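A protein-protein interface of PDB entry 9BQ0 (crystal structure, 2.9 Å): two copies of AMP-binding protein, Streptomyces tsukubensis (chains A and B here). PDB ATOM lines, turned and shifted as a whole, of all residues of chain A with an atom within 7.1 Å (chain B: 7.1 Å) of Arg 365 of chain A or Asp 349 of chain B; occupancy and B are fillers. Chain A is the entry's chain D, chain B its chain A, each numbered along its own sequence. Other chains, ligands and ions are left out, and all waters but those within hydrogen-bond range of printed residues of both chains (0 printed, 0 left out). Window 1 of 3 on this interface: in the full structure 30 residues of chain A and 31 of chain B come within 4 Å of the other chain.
OD1 of Asp 426 of chain A sits at hydrogen-bond distance from N of Asn 429 of chain A, 3.3 Å away.
The backbone NH of Leu 215 of chain B sits at hydrogen-bond distance from the backbone carbonyl oxygen of Arg 210 of chain B (3.1 Å).
OD1 of Asp 426 of chain A sits close to N of Ala 428 of chain A, at 3.3 Å.
The guanidinium group (NH2) of Arg 210 of chain B lies within salt-bridge range of the side-chain carboxylate (OD2) of Asp 349 of chain B.
The backbone NH (N) of Asp 349 of chain B lies within hydrogen-bond range of the backbone carbonyl oxygen (O) of Arg 365 of chain B, 3.0 Å away.
Of the 18 printed residues of chain A, 5 touch a printed residue of chain B.
Printed residues of chain A that touch a printed residue of chain B: Arg 365, Pro 366, Ala 427, Ala 428 and Asn 429.
Hydrophobic or aromatic side chains of chain B that line the printed part of chain A: Leu 215.
Among the printed residues, no Asp or Glu carboxylate lies within 4 Å of a Lys or Arg side-chain nitrogen of the other chain.
Arg 365 of chain A touches just these residues of chain B: Asp 349, Phe 350 and Arg 365.
Of the printed residues of chain A, Asp 349 of chain B touches Arg 365 and Ala 428.
Of the printed residues of chain A, Leu 215 of chain B touches Ala 427 and Asn 429.
Of the printed residues of chain A, Phe 350 of chain B touches Arg 365 (3.6 Å).
Of the printed residues of chain B, Pro 366 of chain A touches Arg 365.
Printed residues of chain B within 4 Å of Asn 429 of chain A: Leu 215 (3.7 Å).
Ala 372 of chain A touches none of the printed residues of chain B.
Arg 210 of chain B touches none of the printed residues of chain A.
The nearest residue of chain B that does not touch Arg 365 of chain A is Gly 364 of chain B (5.7 Å).
The nearest printed residue of chain A that does not touch Asp 349 of chain B is Ala 427 of chain A (4.7 Å).
Among the printed residues, pairs that only touch across the chains: Arg 365 of chain A with Arg 365 of chain B, Ala 427 of chain A with Leu 215 of chain B, Arg 365 of chain A with Phe 350 of chain B, Asn 429 of chain A with Leu 215 of chain B and Ala 428 of chain A with Asp 349 of chain B.
Arg 365 of chain A touches Asp 349 of chain B, but with the chains exchanged Asp 349 of chain A does not touch Arg 365 of chain B (6.0 Å).
Arg 365 of chain A touches Phe 350 of chain B, but with the chains exchanged Phe 350 of chain A does not touch Arg 365 of chain B (8.2 Å).
Arg 365 of chain A touches its own counterpart, Arg 365 of chain B.
Pro 366 of chain A touches Arg 365 of chain B, but with the chains exchanged Arg 365 of chain A does not touch Pro 366 of chain B (6.1 Å).
Of the 7 pairs that touch across the chains among the printed residues, 1 has its exchanged pair printed and touching as well.
The backbone carbonyl oxygen (O) of Asp 349 of chain B lies within hydrogen-bond range of the guanidinium group (NH1) of Arg 365 of chain A.
The backbone carbonyl oxygen (O) of Pro 366 of chain A is in hydrogen-bond range of the guanidinium group (NH2) of Arg 365 of chain B, 2.9 Å away.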
ATOM      1  N   LEU A 347      10.411  41.770  10.748  1.00  0.00           N
ATOM      2  CA  LEU A 347      10.325  40.468  10.121  1.00  0.00           C
ATOM      3  C   LEU A 347      10.673  39.292  11.044  1.00  0.00           C
ATOM      4  O   LEU A 347      10.541  38.133  10.619  1.00  0.00           O
ATOM      5  CB  LEU A 347      11.233  40.436   8.900  1.00  0.00           C
ATOM      6  CG  LEU A 347      10.916  41.420   7.797  1.00  0.00           C
ATOM      7  CD1 LEU A 347      11.530  40.927   6.528  1.00  0.00           C
ATOM      8  CD2 LEU A 347       9.423  41.509   7.740  1.00  0.00           C
ATOM      9  N   PHE A 348      11.128  39.575  12.270  1.00  0.00           N
ATOM     10  CA  PHE A 348      11.483  38.558  13.293  1.00  0.00           C
ATOM     11  C   PHE A 348      11.080  39.057  14.683  1.00  0.00           C
ATOM     12  O   PHE A 348      11.193  40.259  14.918  1.00  0.00           O
ATOM     13  CB  PHE A 348      12.988  38.291  13.344  1.00  0.00           C
ATOM     14  CG  PHE A 348      13.680  37.993  12.042  1.00  0.00           C
ATOM     15  CD1 PHE A 348      13.987  39.008  11.153  1.00  0.00           C
ATOM     16  CD2 PHE A 348      14.087  36.706  11.742  1.00  0.00           C
ATOM     17  CE1 PHE A 348      14.649  38.733   9.968  1.00  0.00           C
ATOM     18  CE2 PHE A 348      14.751  36.433  10.559  1.00  0.00           C
ATOM     19  CZ  PHE A 348      15.029  37.446   9.674  1.00  0.00           C
ATOM     20  N   ASP A 349      10.678  38.164  15.588  1.00  0.00           N
ATOM     21  CA  ASP A 349      10.286  38.512  16.980  1.00  0.00           C
ATOM     22  C   ASP A 349      10.908  37.496  17.948  1.00  0.00           C
ATOM     23  O   ASP A 349      10.710  36.289  17.727  1.00  0.00           O
ATOM     24  CB  ASP A 349       8.763  38.561  17.118  1.00  0.00           C
ATOM     25  CG  ASP A 349       8.250  38.791  18.523  1.00  0.00           C
ATOM     26  OD1 ASP A 349       9.071  39.080  19.401  1.00  0.00           O
ATOM     27  OD2 ASP A 349       7.027  38.693  18.717  1.00  0.00           O
ATOM     28  N   PHE A 350      11.627  37.970  18.972  1.00  0.00           N
ATOM     29  CA  PHE A 350      12.208  37.072  20.003  1.00  0.00           C
ATOM     30  C   PHE A 350      12.147  37.759  21.369  1.00  0.00           C
ATOM     31  O   PHE A 350      11.873  37.059  22.360  1.00  0.00           O
ATOM     32  CB  PHE A 350      13.662  36.737  19.680  1.00  0.00           C
ATOM     33  CG  PHE A 350      14.452  36.204  20.846  1.00  0.00           C
ATOM     34  CD1 PHE A 350      14.134  34.985  21.421  1.00  0.00           C
ATOM     35  CD2 PHE A 350      15.509  36.926  21.376  1.00  0.00           C
ATOM     36  CE1 PHE A 350      14.860  34.499  22.498  1.00  0.00           C
ATOM     37  CE2 PHE A 350      16.234  36.438  22.452  1.00  0.00           C
ATOM     38  CZ  PHE A 350      15.908  35.226  23.011  1.00  0.00           C
ATOM     39  N   CYS A 362      20.379  36.500  19.456  1.00  0.00           N
ATOM     40  CA  CYS A 362      19.221  35.936  18.700  1.00  0.00           C
ATOM     41  C   CYS A 362      18.245  36.996  18.202  1.00  0.00           C
ATOM     42  O   CYS A 362      17.872  37.851  19.013  1.00  0.00           O
ATOM     43  CB  CYS A 362      18.401  34.988  19.565  1.00  0.00           C
ATOM     44  SG  CYS A 362      17.254  33.945  18.627  1.00  0.00           S
ATOM     45  N   ILE A 363      17.814  36.908  16.939  1.00  0.00           N
ATOM     46  CA  ILE A 363      16.815  37.839  16.343  1.00  0.00           C
ATOM     47  C   ILE A 363      15.477  37.108  16.267  1.00  0.00           C
ATOM     48  O   ILE A 363      14.457  37.796  16.174  1.00  0.00           O
ATOM     49  CB  ILE A 363      17.292  38.359  14.977  1.00  0.00           C
ATOM     50  CG1 ILE A 363      17.375  37.256  13.921  1.00  0.00           C
ATOM     51  CG2 ILE A 363      18.618  39.086  15.123  1.00  0.00           C
ATOM     52  CD1 ILE A 363      18.183  37.652  12.709  1.00  0.00           C
ATOM     53  N   GLY A 364      15.475  35.777  16.301  1.00  0.00           N
ATOM     54  CA  GLY A 364      14.245  34.959  16.323  1.00  0.00           C
ATOM     55  C   GLY A 364      13.962  34.270  15.012  1.00  0.00           C
ATOM     56  O   GLY A 364      14.868  34.217  14.200  1.00  0.00           O
ATOM     57  N   ARG A 365      12.738  33.789  14.804  1.00  0.00           N
ATOM     58  CA  ARG A 365      12.306  33.144  13.521  1.00  0.00           C
ATOM     59  C   ARG A 365      11.564  34.145  12.605  1.00  0.00           C
ATOM     60  O   ARG A 365      10.914  35.074  13.095  1.00  0.00           O
ATOM     61  CB  ARG A 365      11.397  31.929  13.752  1.00  0.00           C
ATOM     62  CG  ARG A 365      12.008  30.848  14.612  1.00  0.00           C
ATOM     63  CD  ARG A 365      10.903  29.958  15.256  1.00  0.00           C
ATOM     64  NE  ARG A 365      11.401  28.643  15.658  1.00  0.00           N
ATOM     65  CZ  ARG A 365      10.626  27.623  15.998  1.00  0.00           C
ATOM     66  NH1 ARG A 365       9.304  27.734  16.025  1.00  0.00           N
ATOM     67  NH2 ARG A 365      11.188  26.465  16.335  1.00  0.00           N
ATOM     68  N   PRO A 366      11.717  34.040  11.283  1.00  0.00           N
ATOM     69  CA  PRO A 366      10.988  34.944  10.388  1.00  0.00           C
ATOM     70  C   PRO A 366       9.486  34.776  10.542  1.00  0.00           C
ATOM     71  O   PRO A 366       8.961  33.676  10.728  1.00  0.00           O
ATOM     72  CB  PRO A 366      11.468  34.532   8.994  1.00  0.00           C
ATOM     73  CG  PRO A 366      12.778  33.833   9.216  1.00  0.00           C
ATOM     74  CD  PRO A 366      12.588  33.113  10.540  1.00  0.00           C
ATOM     75  N   MET A 367       8.786  35.881  10.441  1.00  0.00           N
ATOM     76  CA  MET A 367       7.356  35.780  10.603  1.00  0.00           C
ATOM     77  C   MET A 367       6.713  35.390   9.285  1.00  0.00           C
ATOM     78  O   MET A 367       7.243  35.650   8.189  1.00  0.00           O
ATOM     79  CB  MET A 367       6.757  37.090  11.090  1.00  0.00           C
ATOM     80  CG  MET A 367       7.614  37.804  12.048  1.00  0.00           C
ATOM     81  SD  MET A 367       6.875  39.304  12.618  1.00  0.00           S
ATOM     82  CE  MET A 367       8.003  39.757  13.940  1.00  0.00           C
ATOM     83  N   ARG A 368       5.504  34.827   9.433  1.00  0.00           N
ATOM     84  CA  ARG A 368       4.852  34.047   8.383  1.00  0.00           C
ATOM     85  C   ARG A 368       4.774  34.806   7.067  1.00  0.00           C
ATOM     86  O   ARG A 368       4.898  34.189   6.010  1.00  0.00           O
ATOM     87  CB  ARG A 368       3.457  33.593   8.882  1.00  0.00           C
ATOM     88  CG  ARG A 368       2.738  32.614   7.963  1.00  0.00           C
ATOM     89  CD  ARG A 368       1.264  32.433   8.266  1.00  0.00           C
ATOM     90  NE  ARG A 368       0.537  33.690   8.333  1.00  0.00           N
ATOM     91  CZ  ARG A 368      -0.114  34.275   7.333  1.00  0.00           C
ATOM     92  NH1 ARG A 368      -0.434  33.622   6.233  1.00  0.00           N
ATOM     93  NH2 ARG A 368      -0.579  35.515   7.499  1.00  0.00           N
ATOM     94  N   ALA A 372      13.375  34.263   5.072  1.00  0.00           N
ATOM     95  CA  ALA A 372      14.688  34.679   5.518  1.00  0.00           C
ATOM     96  C   ALA A 372      15.712  33.613   5.170  1.00  0.00           C
ATOM     97  O   ALA A 372      15.414  32.408   5.180  1.00  0.00           O
ATOM     98  CB  ALA A 372      14.672  34.952   7.039  1.00  0.00           C
ATOM     99  N   ASP A 426      19.987  28.116  12.784  1.00  0.00           N
ATOM    100  CA  ASP A 426      19.860  26.711  13.146  1.00  0.00           C
ATOM    101  C   ASP A 426      18.819  26.011  12.256  1.00  0.00           C
ATOM    102  O   ASP A 426      18.386  26.548  11.213  1.00  0.00           O
ATOM    103  CB  ASP A 426      19.554  26.601  14.643  1.00  0.00           C
ATOM    104  CG  ASP A 426      18.225  27.230  15.035  1.00  0.00           C
ATOM    105  OD1 ASP A 426      17.552  27.765  14.125  1.00  0.00           O
ATOM    106  OD2 ASP A 426      17.837  27.155  16.241  1.00  0.00           O
ATOM    107  N   ALA A 427      18.497  24.749  12.615  1.00  0.00           N
ATOM    108  CA  ALA A 427      17.522  23.952  11.863  1.00  0.00           C
ATOM    109  C   ALA A 427      16.083  24.463  11.964  1.00  0.00           C
ATOM    110  O   ALA A 427      15.257  24.158  11.090  1.00  0.00           O
ATOM    111  CB  ALA A 427      17.552  22.513  12.357  1.00  0.00           C
ATOM    112  N   ALA A 428      15.751  25.218  13.001  1.00  0.00           N
ATOM    113  CA  ALA A 428      14.415  25.781  13.091  1.00  0.00           C
ATOM    114  C   ALA A 428      14.297  27.094  12.330  1.00  0.00           C
ATOM    115  O   ALA A 428      13.200  27.655  12.251  1.00  0.00           O
ATOM    116  CB  ALA A 428      14.042  25.987  14.557  1.00  0.00           C
ATOM    117  N   ASN A 429      15.366  27.557  11.692  1.00  0.00           N
ATOM    118  CA  ASN A 429      15.377  28.894  11.114  1.00  0.00           C
ATOM    119  C   ASN A 429      15.256  29.978  12.193  1.00  0.00           C
ATOM    120  O   ASN A 429      14.541  30.981  12.034  1.00  0.00           O
ATOM    121  CB  ASN A 429      14.270  28.993  10.076  1.00  0.00           C
ATOM    122  CG  ASN A 429      14.774  29.455   8.754  1.00  0.00           C
ATOM    123  OD1 ASN A 429      15.909  29.165   8.355  1.00  0.00           O
ATOM    124  ND2 ASN A 429      13.926  30.178   8.041  1.00  0.00           N
ATOM    125  N   THR A 430      15.919  29.740  13.332  1.00  0.00           N
ATOM    126  CA  THR A 430      16.217  30.789  14.307  1.00  0.00           C
ATOM    127  C   THR A 430      17.543  31.453  13.929  1.00  0.00           C
ATOM    128  O   THR A 430      18.578  30.791  13.885  1.00  0.00           O
ATOM    129  CB  THR A 430      16.294  30.230  15.728  1.00  0.00           C
ATOM    130  OG1 THR A 430      15.013  29.792  16.136  1.00  0.00           O
ATOM    131  CG2 THR A 430      16.754  31.292  16.660  1.00  0.00           C
ATOM    132  N   PHE A 431      17.499  32.756  13.682  1.00  0.00           N
ATOM    133  CA  PHE A 431      18.642  33.543  13.235  1.00  0.00           C
ATOM    134  C   PHE A 431      19.328  34.282  14.398  1.00  0.00           C
ATOM    135  O   PHE A 431      18.717  34.570  15.438  1.00  0.00           O
ATOM    136  CB  PHE A 431      18.184  34.511  12.130  1.00  0.00           C
ATOM    137  CG  PHE A 431      17.733  33.814  10.862  1.00  0.00           C
ATOM    138  CD1 PHE A 431      16.545  33.128  10.817  1.00  0.00           C
ATOM    139  CD2 PHE A 431      18.501  33.829   9.740  1.00  0.00           C
ATOM    140  CE1 PHE A 431      16.129  32.473   9.678  1.00  0.00           C
ATOM    141  CE2 PHE A 431      18.079  33.177   8.613  1.00  0.00           C
ATOM    142  CZ  PHE A 431      16.878  32.497   8.593  1.00  0.00           C
ATOM    143  N   ARG B 210       9.263  24.249   2.446  1.00  0.00           N
ATOM    144  CA  ARG B 210      10.345  24.221   3.417  1.00  0.00           C
ATOM    145  C   ARG B 210      11.691  24.206   2.719  1.00  0.00           C
ATOM    146  O   ARG B 210      12.542  25.058   2.991  1.00  0.00           O
ATOM    147  CB  ARG B 210      10.206  23.013   4.334  1.00  0.00           C
ATOM    148  CG  ARG B 210       9.159  23.204   5.359  1.00  0.00           C
ATOM    149  CD  ARG B 210       9.383  22.411   6.612  1.00  0.00           C
ATOM    150  NE  ARG B 210      10.486  22.846   7.463  1.00  0.00           N
ATOM    151  CZ  ARG B 210      10.452  23.941   8.211  1.00  0.00           C
ATOM    152  NH1 ARG B 210       9.426  24.771   8.166  1.00  0.00           N
ATOM    153  NH2 ARG B 210      11.441  24.184   9.068  1.00  0.00           N
ATOM    154  N   LEU B 215      15.165  24.267   4.541  1.00  0.00           N
ATOM    155  CA  LEU B 215      14.816  23.432   5.667  1.00  0.00           C
ATOM    156  C   LEU B 215      14.325  22.077   5.189  1.00  0.00           C
ATOM    157  O   LEU B 215      14.028  21.891   4.009  1.00  0.00           O
ATOM    158  CB  LEU B 215      13.779  24.132   6.506  1.00  0.00           C
ATOM    159  CG  LEU B 215      14.287  25.516   6.930  1.00  0.00           C
ATOM    160  CD1 LEU B 215      13.052  26.400   6.862  1.00  0.00           C
ATOM    161  CD2 LEU B 215      14.988  25.587   8.328  1.00  0.00           C
ATOM    162  N   ASP B 216      14.285  21.127   6.136  1.00  0.00           N
ATOM    163  CA  ASP B 216      13.908  19.726   5.943  1.00  0.00           C
ATOM    164  C   ASP B 216      14.431  19.132   4.649  1.00  0.00           C
ATOM    165  O   ASP B 216      13.790  18.258   4.077  1.00  0.00           O
ATOM    166  CB  ASP B 216      12.393  19.592   5.982  1.00  0.00           C
ATOM    167  CG  ASP B 216      11.845  19.915   7.310  1.00  0.00           C
ATOM    168  OD1 ASP B 216      12.660  20.087   8.215  1.00  0.00           O
ATOM    169  OD2 ASP B 216      10.619  19.976   7.502  1.00  0.00           O
ATOM    170  N   TYR B 297      11.758  11.298  15.133  1.00  0.00           N
ATOM    171  CA  TYR B 297      10.545  12.023  14.684  1.00  0.00           C
ATOM    172  C   TYR B 297       9.285  11.203  14.926  1.00  0.00           C
ATOM    173  O   TYR B 297       9.080  10.244  14.190  1.00  0.00           O
ATOM    174  CB  TYR B 297      10.623  12.310  13.190  1.00  0.00           C
ATOM    175  CG  TYR B 297      11.660  13.313  12.766  1.00  0.00           C
ATOM    176  CD1 TYR B 297      11.377  14.665  12.763  1.00  0.00           C
ATOM    177  CD2 TYR B 297      12.906  12.908  12.326  1.00  0.00           C
ATOM    178  CE1 TYR B 297      12.318  15.597  12.368  1.00  0.00           C
ATOM    179  CE2 TYR B 297      13.857  13.827  11.919  1.00  0.00           C
ATOM    180  CZ  TYR B 297      13.564  15.175  11.946  1.00  0.00           C
ATOM    181  OH  TYR B 297      14.501  16.080  11.549  1.00  0.00           O
ATOM    182  N   ILE B 335      11.384  15.182  18.075  1.00  0.00           N
ATOM    183  CA  ILE B 335      10.399  16.014  17.391  1.00  0.00           C
ATOM    184  C   ILE B 335       9.068  15.290  17.408  1.00  0.00           C
ATOM    185  O   ILE B 335       8.856  14.379  16.615  1.00  0.00           O
ATOM    186  CB  ILE B 335      10.798  16.292  15.948  1.00  0.00           C
ATOM    187  CG1 ILE B 335      12.266  16.602  15.904  1.00  0.00           C
ATOM    188  CG2 ILE B 335       9.990  17.397  15.419  1.00  0.00           C
ATOM    189  CD1 ILE B 335      13.034  15.389  15.603  1.00  0.00           C
ATOM    190  N   MET B 337       5.800  15.485  16.043  1.00  0.00           N
ATOM    191  CA  MET B 337       5.148  16.314  15.012  1.00  0.00           C
ATOM    192  C   MET B 337       3.643  16.123  15.183  1.00  0.00           C
ATOM    193  O   MET B 337       3.256  15.069  15.709  1.00  0.00           O
ATOM    194  CB  MET B 337       5.637  15.929  13.618  1.00  0.00           C
ATOM    195  CG  MET B 337       7.102  15.582  13.574  1.00  0.00           C
ATOM    196  SD  MET B 337       7.663  15.313  11.891  1.00  0.00           S
ATOM    197  CE  MET B 337       8.267  16.956  11.516  1.00  0.00           C
ATOM    198  N   VAL B 346       3.712  18.340   7.961  1.00  0.00           N
ATOM    199  CA  VAL B 346       3.593  18.929   9.273  1.00  0.00           C
ATOM    200  C   VAL B 346       3.340  20.408   9.107  1.00  0.00           C
ATOM    201  O   VAL B 346       3.800  21.019   8.143  1.00  0.00           O
ATOM    202  CB  VAL B 346       4.845  18.573  10.072  1.00  0.00           C
ATOM    203  CG1 VAL B 346       4.541  17.209  10.641  1.00  0.00           C
ATOM    204  CG2 VAL B 346       6.095  18.613   9.149  1.00  0.00           C
ATOM    205  N   LEU B 347       2.496  20.950   9.980  1.00  0.00           N
ATOM    206  CA  LEU B 347       2.160  22.365   9.950  1.00  0.00           C
ATOM    207  C   LEU B 347       2.777  23.109  11.118  1.00  0.00           C
ATOM    208  O   LEU B 347       2.898  24.338  11.066  1.00  0.00           O
ATOM    209  CB  LEU B 347       0.629  22.566   9.949  1.00  0.00           C
ATOM    210  CG  LEU B 347      -0.246  21.651   9.072  1.00  0.00           C
ATOM    211  CD1 LEU B 347      -1.719  21.590   9.538  1.00  0.00           C
ATOM    212  CD2 LEU B 347      -0.110  22.118   7.608  1.00  0.00           C
ATOM    213  N   PHE B 348       3.306  22.389  12.090  1.00  0.00           N
ATOM    214  CA  PHE B 348       3.873  22.993  13.279  1.00  0.00           C
ATOM    215  C   PHE B 348       5.298  22.509  13.523  1.00  0.00           C
ATOM    216  O   PHE B 348       5.574  21.302  13.529  1.00  0.00           O
ATOM    217  CB  PHE B 348       3.026  22.620  14.463  1.00  0.00           C
ATOM    218  CG  PHE B 348       1.686  23.313  14.535  1.00  0.00           C
ATOM    219  CD1 PHE B 348       1.578  24.596  15.022  1.00  0.00           C
ATOM    220  CD2 PHE B 348       0.531  22.644  14.176  1.00  0.00           C
ATOM    221  CE1 PHE B 348       0.332  25.187  15.129  1.00  0.00           C
ATOM    222  CE2 PHE B 348      -0.709  23.226  14.294  1.00  0.00           C
ATOM    223  CZ  PHE B 348      -0.816  24.476  14.750  1.00  0.00           C
ATOM    224  N   ASP B 349       6.184  23.462  13.814  1.00  0.00           N
ATOM    225  CA  ASP B 349       7.615  23.194  14.072  1.00  0.00           C
ATOM    226  C   ASP B 349       8.014  23.731  15.440  1.00  0.00           C
ATOM    227  O   ASP B 349       7.817  24.925  15.645  1.00  0.00           O
ATOM    228  CB  ASP B 349       8.463  23.933  13.042  1.00  0.00           C
ATOM    229  CG  ASP B 349       9.879  23.427  12.866  1.00  0.00           C
ATOM    230  OD1 ASP B 349      10.090  22.210  12.993  1.00  0.00           O
ATOM    231  OD2 ASP B 349      10.760  24.264  12.597  1.00  0.00           O
ATOM    232  N   PHE B 350       8.610  22.924  16.321  1.00  0.00           N
ATOM    233  CA  PHE B 350       9.151  23.414  17.621  1.00  0.00           C
ATOM    234  C   PHE B 350      10.665  23.191  17.657  1.00  0.00           C
ATOM    235  O   PHE B 350      11.275  23.691  18.614  1.00  0.00           O
ATOM    236  CB  PHE B 350       8.462  22.746  18.810  1.00  0.00           C
ATOM    237  CG  PHE B 350       8.805  21.298  19.029  1.00  0.00           C
ATOM    238  CD1 PHE B 350       8.193  20.306  18.284  1.00  0.00           C
ATOM    239  CD2 PHE B 350       9.717  20.928  20.001  1.00  0.00           C
ATOM    240  CE1 PHE B 350       8.503  18.973  18.495  1.00  0.00           C
ATOM    241  CE2 PHE B 350      10.028  19.595  20.210  1.00  0.00           C
ATOM    242  CZ  PHE B 350       9.417  18.622  19.461  1.00  0.00           C
ATOM    243  N   CYS B 362       3.442  20.432  23.751  1.00  0.00           N
ATOM    244  CA  CYS B 362       3.714  21.505  22.804  1.00  0.00           C
ATOM    245  C   CYS B 362       3.642  20.870  21.421  1.00  0.00           C
ATOM    246  O   CYS B 362       4.246  19.813  21.202  1.00  0.00           O
ATOM    247  CB  CYS B 362       5.084  22.150  23.056  1.00  0.00           C
ATOM    248  SG  CYS B 362       5.462  23.741  22.177  1.00  0.00           S
ATOM    249  N   ILE B 363       2.811  21.418  20.536  1.00  0.00           N
ATOM    250  CA  ILE B 363       2.815  20.918  19.186  1.00  0.00           C
ATOM    251  C   ILE B 363       3.742  21.688  18.258  1.00  0.00           C
ATOM    252  O   ILE B 363       4.222  21.093  17.274  1.00  0.00           O
ATOM    253  CB  ILE B 363       1.397  20.869  18.623  1.00  0.00           C
ATOM    254  CG1 ILE B 363       0.842  22.249  18.482  1.00  0.00           C
ATOM    255  CG2 ILE B 363       0.471  20.108  19.527  1.00  0.00           C
ATOM    256  CD1 ILE B 363      -0.705  22.200  18.411  1.00  0.00           C
ATOM    257  N   GLY B 364       4.080  22.955  18.583  1.00  0.00           N
ATOM    258  CA  GLY B 364       4.975  23.826  17.818  1.00  0.00           C
ATOM    259  C   GLY B 364       4.386  25.192  17.465  1.00  0.00           C
ATOM    260  O   GLY B 364       3.424  25.678  18.067  1.00  0.00           O
ATOM    261  N   ARG B 365       5.036  25.851  16.549  1.00  0.00           N
ATOM    262  CA  ARG B 365       4.718  27.140  15.963  1.00  0.00           C
ATOM    263  C   ARG B 365       4.250  26.935  14.533  1.00  0.00           C
ATOM    264  O   ARG B 365       4.790  26.078  13.839  1.00  0.00           O
ATOM    265  CB  ARG B 365       5.961  28.049  15.985  1.00  0.00           C
ATOM    266  CG  ARG B 365       5.724  29.428  15.442  1.00  0.00           C
ATOM    267  CD  ARG B 365       6.954  30.286  15.646  1.00  0.00           C
ATOM    268  NE  ARG B 365       7.740  30.446  14.424  1.00  0.00           N
ATOM    269  CZ  ARG B 365       7.932  31.610  13.820  1.00  0.00           C
ATOM    270  NH1 ARG B 365       7.370  32.722  14.268  1.00  0.00           N
ATOM    271  NH2 ARG B 365       8.710  31.664  12.747  1.00  0.00           N
ATOM    272  N   PRO B 366       3.277  27.686  14.038  1.00  0.00           N
ATOM    273  CA  PRO B 366       2.831  27.435  12.672  1.00  0.00           C
ATOM    274  C   PRO B 366       3.982  27.633  11.680  1.00  0.00           C
ATOM    275  O   PRO B 366       4.886  28.450  11.873  1.00  0.00           O
ATOM    276  CB  PRO B 366       1.697  28.432  12.497  1.00  0.00           C
ATOM    277  CG  PRO B 366       1.323  28.819  13.916  1.00  0.00           C
ATOM    278  CD  PRO B 366       2.582  28.836  14.625  1.00  0.00           C
ATOM    279  N   MET B 367       4.016  26.781  10.683  1.00  0.00           N
ATOM    280  CA  MET B 367       5.033  26.820   9.650  1.00  0.00           C
ATOM    281  C   MET B 367       4.571  27.784   8.548  1.00  0.00           C
ATOM    282  O   MET B 367       3.381  28.084   8.421  1.00  0.00           O
ATOM    283  CB  MET B 367       5.277  25.383   9.186  1.00  0.00           C
ATOM    284  CG  MET B 367       6.657  24.853   9.412  1.00  0.00           C
ATOM    285  SD  MET B 367       6.599  23.151   8.945  1.00  0.00           S
ATOM    286  CE  MET B 367       8.010  22.487   9.800  1.00  0.00           C
ATOM    287  N   THR B 430       2.730  30.066  20.009  1.00  0.00           N
ATOM    288  CA  THR B 430       3.051  28.675  20.245  1.00  0.00           C
ATOM    289  C   THR B 430       1.845  27.915  20.765  1.00  0.00           C
ATOM    290  O   THR B 430       1.244  28.314  21.766  1.00  0.00           O
ATOM    291  CB  THR B 430       4.205  28.549  21.211  1.00  0.00           C
ATOM    292  OG1 THR B 430       5.260  29.276  20.605  1.00  0.00           O
ATOM    293  CG2 THR B 430       4.566  27.029  21.456  1.00  0.00           C
